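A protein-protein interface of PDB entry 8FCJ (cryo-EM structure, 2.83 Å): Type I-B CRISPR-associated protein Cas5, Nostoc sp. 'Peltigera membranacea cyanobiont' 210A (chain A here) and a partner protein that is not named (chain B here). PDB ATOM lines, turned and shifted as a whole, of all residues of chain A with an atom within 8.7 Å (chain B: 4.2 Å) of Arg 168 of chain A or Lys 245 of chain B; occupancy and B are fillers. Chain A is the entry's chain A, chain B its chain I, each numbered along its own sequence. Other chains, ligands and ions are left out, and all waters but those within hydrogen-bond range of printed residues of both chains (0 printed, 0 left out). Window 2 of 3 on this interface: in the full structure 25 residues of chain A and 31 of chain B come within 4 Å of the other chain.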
ATOM      1  N   ILE A 164      10.947 -25.335 -21.553  1.00  0.00           N
ATOM      2  CA  ILE A 164       9.691 -25.088 -20.859  1.00  0.00           C
ATOM      3  C   ILE A 164       8.932 -23.992 -21.589  1.00  0.00           C
ATOM      4  O   ILE A 164       9.505 -22.952 -21.932  1.00  0.00           O
ATOM      5  CB  ILE A 164       9.934 -24.694 -19.393  1.00  0.00           C
ATOM      6  CG1 ILE A 164      11.080 -25.512 -18.802  1.00  0.00           C
ATOM      7  CG2 ILE A 164       8.669 -24.882 -18.578  1.00  0.00           C
ATOM      8  CD1 ILE A 164      10.699 -26.921 -18.453  1.00  0.00           C
ATOM      9  N   ARG A 165       7.644 -24.219 -21.822  1.00  0.00           N
ATOM     10  CA  ARG A 165       6.795 -23.218 -22.463  1.00  0.00           C
ATOM     11  C   ARG A 165       6.560 -22.079 -21.483  1.00  0.00           C
ATOM     12  O   ARG A 165       5.708 -22.170 -20.597  1.00  0.00           O
ATOM     13  CB  ARG A 165       5.475 -23.838 -22.905  1.00  0.00           C
ATOM     14  CG  ARG A 165       5.538 -24.563 -24.230  1.00  0.00           C
ATOM     15  CD  ARG A 165       4.166 -25.052 -24.636  1.00  0.00           C
ATOM     16  NE  ARG A 165       3.473 -25.690 -23.526  1.00  0.00           N
ATOM     17  CZ  ARG A 165       2.197 -26.048 -23.546  1.00  0.00           C
ATOM     18  NH1 ARG A 165       1.441 -25.844 -24.612  1.00  0.00           N
ATOM     19  NH2 ARG A 165       1.668 -26.625 -22.472  1.00  0.00           N
ATOM     20  N   ASP A 166       7.316 -20.998 -21.638  1.00  0.00           N
ATOM     21  CA  ASP A 166       7.205 -19.827 -20.783  1.00  0.00           C
ATOM     22  C   ASP A 166       6.824 -18.646 -21.661  1.00  0.00           C
ATOM     23  O   ASP A 166       7.484 -18.379 -22.670  1.00  0.00           O
ATOM     24  CB  ASP A 166       8.526 -19.565 -20.047  1.00  0.00           C
ATOM     25  CG  ASP A 166       8.485 -18.337 -19.141  1.00  0.00           C
ATOM     26  OD1 ASP A 166       7.597 -17.470 -19.284  1.00  0.00           O
ATOM     27  OD2 ASP A 166       9.353 -18.253 -18.249  1.00  0.00           O
ATOM     28  N   ASN A 167       5.761 -17.938 -21.276  1.00  0.00           N
ATOM     29  CA  ASN A 167       5.322 -16.784 -22.050  1.00  0.00           C
ATOM     30  C   ASN A 167       6.308 -15.627 -21.975  1.00  0.00           C
ATOM     31  O   ASN A 167       6.237 -14.717 -22.806  1.00  0.00           O
ATOM     32  CB  ASN A 167       3.942 -16.331 -21.577  1.00  0.00           C
ATOM     33  CG  ASN A 167       2.821 -17.030 -22.313  1.00  0.00           C
ATOM     34  OD1 ASN A 167       3.060 -17.802 -23.241  1.00  0.00           O
ATOM     35  ND2 ASN A 167       1.586 -16.766 -21.903  1.00  0.00           N
ATOM     36  N   ARG A 168       7.218 -15.638 -21.004  1.00  0.00           N
ATOM     37  CA  ARG A 168       8.288 -14.655 -20.918  1.00  0.00           C
ATOM     38  C   ARG A 168       9.614 -15.197 -21.429  1.00  0.00           C
ATOM     39  O   ARG A 168      10.656 -14.574 -21.205  1.00  0.00           O
ATOM     40  CB  ARG A 168       8.450 -14.167 -19.477  1.00  0.00           C
ATOM     41  CG  ARG A 168       7.178 -14.218 -18.656  1.00  0.00           C
ATOM     42  CD  ARG A 168       6.246 -13.087 -19.034  1.00  0.00           C
ATOM     43  NE  ARG A 168       6.851 -11.780 -18.808  1.00  0.00           N
ATOM     44  CZ  ARG A 168       6.663 -10.724 -19.589  1.00  0.00           C
ATOM     45  NH1 ARG A 168       5.893 -10.786 -20.662  1.00  0.00           N
ATOM     46  NH2 ARG A 168       7.263  -9.577 -19.285  1.00  0.00           N
ATOM     47  N   GLY A 169       9.600 -16.342 -22.105  1.00  0.00           N
ATOM     48  CA  GLY A 169      10.834 -16.951 -22.546  1.00  0.00           C
ATOM     49  C   GLY A 169      11.474 -16.210 -23.702  1.00  0.00           C
ATOM     50  O   GLY A 169      10.861 -15.385 -24.377  1.00  0.00           O
ATOM     51  N   ARG A 170      12.749 -16.525 -23.927  1.00  0.00           N
ATOM     52  CA  ARG A 170      13.505 -15.893 -25.002  1.00  0.00           C
ATOM     53  C   ARG A 170      13.182 -16.519 -26.351  1.00  0.00           C
ATOM     54  O   ARG A 170      12.825 -15.816 -27.301  1.00  0.00           O
ATOM     55  CB  ARG A 170      15.003 -16.006 -24.721  1.00  0.00           C
ATOM     56  CG  ARG A 170      15.551 -14.982 -23.751  1.00  0.00           C
ATOM     57  CD  ARG A 170      17.034 -15.217 -23.497  1.00  0.00           C
ATOM     58  NE  ARG A 170      17.777 -15.439 -24.733  1.00  0.00           N
ATOM     59  CZ  ARG A 170      18.278 -16.609 -25.106  1.00  0.00           C
ATOM     60  NH1 ARG A 170      18.133 -17.693 -24.362  1.00  0.00           N
ATOM     61  NH2 ARG A 170      18.938 -16.695 -26.259  1.00  0.00           N
ATOM     62  N   LEU A 171      13.309 -17.838 -26.451  1.00  0.00           N
ATOM     63  CA  LEU A 171      13.166 -18.516 -27.731  1.00  0.00           C
ATOM     64  C   LEU A 171      11.720 -18.497 -28.202  1.00  0.00           C
ATOM     65  O   LEU A 171      10.786 -18.598 -27.403  1.00  0.00           O
ATOM     66  CB  LEU A 171      13.654 -19.957 -27.622  1.00  0.00           C
ATOM     67  CG  LEU A 171      14.862 -20.190 -26.719  1.00  0.00           C
ATOM     68  CD1 LEU A 171      15.147 -21.671 -26.602  1.00  0.00           C
ATOM     69  CD2 LEU A 171      16.072 -19.454 -27.258  1.00  0.00           C
ATOM     70  N   THR A 172      11.541 -18.366 -29.512  1.00  0.00           N
ATOM     71  CA  THR A 172      10.232 -18.436 -30.155  1.00  0.00           C
ATOM     72  C   THR A 172      10.312 -19.554 -31.187  1.00  0.00           C
ATOM     73  O   THR A 172      10.588 -19.311 -32.363  1.00  0.00           O
ATOM     74  CB  THR A 172       9.851 -17.107 -30.791  1.00  0.00           C
ATOM     75  OG1 THR A 172      10.101 -16.045 -29.863  1.00  0.00           O
ATOM     76  CG2 THR A 172       8.384 -17.101 -31.166  1.00  0.00           C
ATOM     77  N   ARG A 189       6.535 -19.638 -27.229  1.00  0.00           N
ATOM     78  CA  ARG A 189       7.713 -19.115 -26.552  1.00  0.00           C
ATOM     79  C   ARG A 189       8.197 -20.107 -25.504  1.00  0.00           C
ATOM     80  O   ARG A 189       7.404 -20.616 -24.707  1.00  0.00           O
ATOM     81  CB  ARG A 189       7.415 -17.763 -25.908  1.00  0.00           C
ATOM     82  CG  ARG A 189       7.615 -16.586 -26.841  1.00  0.00           C
ATOM     83  CD  ARG A 189       6.827 -15.386 -26.371  1.00  0.00           C
ATOM     84  NE  ARG A 189       7.475 -14.717 -25.250  1.00  0.00           N
ATOM     85  CZ  ARG A 189       7.678 -13.410 -25.178  1.00  0.00           C
ATOM     86  NH1 ARG A 189       7.279 -12.596 -26.139  1.00  0.00           N
ATOM     87  NH2 ARG A 189       8.292 -12.908 -24.111  1.00  0.00           N
ATOM     88  N   TYR A 190       9.500 -20.368 -25.503  1.00  0.00           N
ATOM     89  CA  TYR A 190      10.110 -21.357 -24.630  1.00  0.00           C
ATOM     90  C   TYR A 190      11.240 -20.729 -23.827  1.00  0.00           C
ATOM     91  O   TYR A 190      11.736 -19.645 -24.140  1.00  0.00           O
ATOM     92  CB  TYR A 190      10.653 -22.546 -25.430  1.00  0.00           C
ATOM     93  CG  TYR A 190       9.601 -23.343 -26.159  1.00  0.00           C
ATOM     94  CD1 TYR A 190       9.056 -22.881 -27.346  1.00  0.00           C
ATOM     95  CD2 TYR A 190       9.159 -24.558 -25.665  1.00  0.00           C
ATOM     96  CE1 TYR A 190       8.099 -23.602 -28.015  1.00  0.00           C
ATOM     97  CE2 TYR A 190       8.202 -25.287 -26.329  1.00  0.00           C
ATOM     98  CZ  TYR A 190       7.675 -24.802 -27.502  1.00  0.00           C
ATOM     99  OH  TYR A 190       6.719 -25.521 -28.173  1.00  0.00           O
ATOM    100  N   ARG A 191      11.641 -21.438 -22.776  1.00  0.00           N
ATOM    101  CA  ARG A 191      12.838 -21.114 -22.019  1.00  0.00           C
ATOM    102  C   ARG A 191      13.570 -22.409 -21.709  1.00  0.00           C
ATOM    103  O   ARG A 191      12.968 -23.483 -21.646  1.00  0.00           O
ATOM    104  CB  ARG A 191      12.513 -20.353 -20.727  1.00  0.00           C
ATOM    105  CG  ARG A 191      12.522 -21.210 -19.476  1.00  0.00           C
ATOM    106  CD  ARG A 191      11.622 -20.627 -18.407  1.00  0.00           C
ATOM    107  NE  ARG A 191      11.310 -21.602 -17.371  1.00  0.00           N
ATOM    108  CZ  ARG A 191      10.128 -21.710 -16.779  1.00  0.00           C
ATOM    109  NH1 ARG A 191       9.119 -20.917 -17.100  1.00  0.00           N
ATOM    110  NH2 ARG A 191       9.954 -22.639 -15.844  1.00  0.00           N
ATOM    111  N   LEU B  21       3.545  -7.975 -24.142  1.00  0.00           N
ATOM    112  CA  LEU B  21       4.822  -8.676 -24.118  1.00  0.00           C
ATOM    113  C   LEU B  21       4.654 -10.162 -23.843  1.00  0.00           C
ATOM    114  O   LEU B  21       5.555 -10.945 -24.159  1.00  0.00           O
ATOM    115  CB  LEU B  21       5.742  -8.068 -23.060  1.00  0.00           C
ATOM    116  CG  LEU B  21       6.375  -6.712 -23.356  1.00  0.00           C
ATOM    117  CD1 LEU B  21       7.179  -6.238 -22.162  1.00  0.00           C
ATOM    118  CD2 LEU B  21       7.251  -6.801 -24.583  1.00  0.00           C
ATOM    119  N   HIS B  22       3.526 -10.565 -23.260  1.00  0.00           N
ATOM    120  CA  HIS B  22       3.295 -11.955 -22.901  1.00  0.00           C
ATOM    121  C   HIS B  22       2.740 -12.784 -24.048  1.00  0.00           C
ATOM    122  O   HIS B  22       2.548 -13.992 -23.876  1.00  0.00           O
ATOM    123  CB  HIS B  22       2.338 -12.033 -21.710  1.00  0.00           C
ATOM    124  CG  HIS B  22       2.800 -11.265 -20.512  1.00  0.00           C
ATOM    125  ND1 HIS B  22       3.243 -11.878 -19.360  1.00  0.00           N
ATOM    126  CD2 HIS B  22       2.889  -9.932 -20.286  1.00  0.00           C
ATOM    127  CE1 HIS B  22       3.583 -10.957 -18.477  1.00  0.00           C
ATOM    128  NE2 HIS B  22       3.381  -9.769 -19.015  1.00  0.00           N
ATOM    129  N   GLU B 243      16.816  -7.125 -25.484  1.00  0.00           N
ATOM    130  CA  GLU B 243      15.753  -8.044 -25.102  1.00  0.00           C
ATOM    131  C   GLU B 243      14.903  -7.373 -24.032  1.00  0.00           C
ATOM    132  O   GLU B 243      15.403  -7.044 -22.951  1.00  0.00           O
ATOM    133  CB  GLU B 243      16.329  -9.364 -24.596  1.00  0.00           C
ATOM    134  CG  GLU B 243      17.178 -10.090 -25.621  1.00  0.00           C
ATOM    135  CD  GLU B 243      17.066 -11.594 -25.504  1.00  0.00           C
ATOM    136  OE1 GLU B 243      16.856 -12.087 -24.377  1.00  0.00           O
ATOM    137  OE2 GLU B 243      17.188 -12.283 -26.538  1.00  0.00           O
ATOM    138  N   ILE B 244      13.625  -7.174 -24.332  1.00  0.00           N
ATOM    139  CA  ILE B 244      12.760  -6.351 -23.495  1.00  0.00           C
ATOM    140  C   ILE B 244      12.240  -7.181 -22.329  1.00  0.00           C
ATOM    141  O   ILE B 244      11.649  -8.247 -22.525  1.00  0.00           O
ATOM    142  CB  ILE B 244      11.602  -5.765 -24.311  1.00  0.00           C
ATOM    143  CG1 ILE B 244      12.137  -5.052 -25.551  1.00  0.00           C
ATOM    144  CG2 ILE B 244      10.786  -4.817 -23.460  1.00  0.00           C
ATOM    145  CD1 ILE B 244      13.068  -3.912 -25.239  1.00  0.00           C
ATOM    146  N   LYS B 245      12.459  -6.688 -21.112  1.00  0.00           N
ATOM    147  CA  LYS B 245      11.857  -7.263 -19.918  1.00  0.00           C
ATOM    148  C   LYS B 245      10.645  -6.484 -19.437  1.00  0.00           C
ATOM    149  O   LYS B 245       9.737  -7.072 -18.843  1.00  0.00           O
ATOM    150  CB  LYS B 245      12.883  -7.332 -18.782  1.00  0.00           C
ATOM    151  CG  LYS B 245      14.002  -8.327 -19.013  1.00  0.00           C
ATOM    152  CD  LYS B 245      14.737  -8.624 -17.719  1.00  0.00           C
ATOM    153  CE  LYS B 245      15.702  -9.784 -17.888  1.00  0.00           C
ATOM    154  NZ  LYS B 245      16.263 -10.223 -16.581  1.00  0.00           N
ATOM    155  N   ASP B 246      10.616  -5.179 -19.685  1.00  0.00           N
ATOM    156  CA  ASP B 246       9.515  -4.326 -19.271  1.00  0.00           C
ATOM    157  C   ASP B 246       9.535  -3.081 -20.141  1.00  0.00           C
ATOM    158  O   ASP B 246      10.606  -2.623 -20.544  1.00  0.00           O
ATOM    159  CB  ASP B 246       9.632  -3.948 -17.792  1.00  0.00           C
ATOM    160  CG  ASP B 246       8.343  -4.157 -17.034  1.00  0.00           C
ATOM    161  OD1 ASP B 246       7.266  -4.050 -17.654  1.00  0.00           O
ATOM    162  OD2 ASP B 246       8.405  -4.430 -15.817  1.00  0.00           O
ATOM    163  N   TYR B 290      20.303  -8.978 -14.666  1.00  0.00           N
ATOM    164  CA  TYR B 290      20.485  -9.825 -15.842  1.00  0.00           C
ATOM    165  C   TYR B 290      19.836  -9.140 -17.031  1.00  0.00           C
ATOM    166  O   TYR B 290      18.640  -8.837 -16.991  1.00  0.00           O
ATOM    167  CB  TYR B 290      19.881 -11.209 -15.629  1.00  0.00           C
ATOM    168  CG  TYR B 290      19.816 -12.023 -16.898  1.00  0.00           C
ATOM    169  CD1 TYR B 290      20.972 -12.499 -17.498  1.00  0.00           C
ATOM    170  CD2 TYR B 290      18.600 -12.304 -17.505  1.00  0.00           C
ATOM    171  CE1 TYR B 290      20.920 -13.239 -18.662  1.00  0.00           C
ATOM    172  CE2 TYR B 290      18.537 -13.042 -18.668  1.00  0.00           C
ATOM    173  CZ  TYR B 290      19.700 -13.507 -19.242  1.00  0.00           C
ATOM    174  OH  TYR B 290      19.644 -14.244 -20.402  1.00  0.00           O
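The guanidinium group (NH1) of Arg 168 of chain A lies close to a ring nitrogen (ND1) of His 22 of chain B (3.1 Å).
OE1 of Glu 243 of chain B lies within salt-bridge range of NE of Arg 170 of chain A (3.5 Å).
NH1 of Arg 189 of chain A is in hydrogen-bond range of O of Leu 21 of chain B (3.1 Å).
N of Arg 170 of chain A is in hydrogen-bond range of O of Tyr 190 of chain A (3.3 Å).
The backbone carbonyl oxygen of Tyr 290 of chain B is in hydrogen-bond range of the side-chain amino group of Lys 245 of chain B.
N of Asp 166 of chain A is in hydrogen-bond range of O of Arg 189 of chain A.
The guanidinium group (NE) of Arg 189 of chain A is in hydrogen-bond range of the backbone carbonyl oxygen (O) of Asn 167 of chain A, 2.7 Å away.
OD1 of Asp 166 of chain A is in hydrogen-bond range of N of Arg 168 of chain A (2.5 Å).
CG of Asn 167 of chain A touches O of His 22 of chain B, at 3.4 Å.
Leu 21 of chain B touches Arg 168 of chain A (C to NH1, 3.5 Å).
Arg 168 of chain A touches Lys 245 of chain B (NH2 to O, 3.5 Å).
Lys 245 of chain B touches just one residue of chain A: Arg 168 (3.5 Å).
Asp 246 of chain B touches none of the printed residues of chain A.
Printed residues of chain A within 4 Å of His 22 of chain B: Asn 167 and Arg 168.
Of the printed residues of chain A, Leu 21 of chain B touches Arg 168 and Arg 189.
Tyr 190 of chain A touches none of the printed residues of chain B.
The nearest residue of chain A that does not touch Lys 245 of chain B is Arg 170 of chain A (7.8 Å).
Of the 7 printed residues of chain B, 4 touch a printed residue of chain A.
Printed residues of chain B that touch a printed residue of chain A: Leu 21, His 22, Glu 243 and Lys 245.
Hydrophobic or aromatic side chains of chain B that line the printed part of chain A: Leu 21 and His 22.
Among the printed residues, 6 pairs touch across the chains.
Among the printed residues, Asp or Glu carboxylates within 4 Å of a Lys or Arg side-chain nitrogen of the other chain: Arg 170 of chain A with Glu 243 of chain B (3.5 Å).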
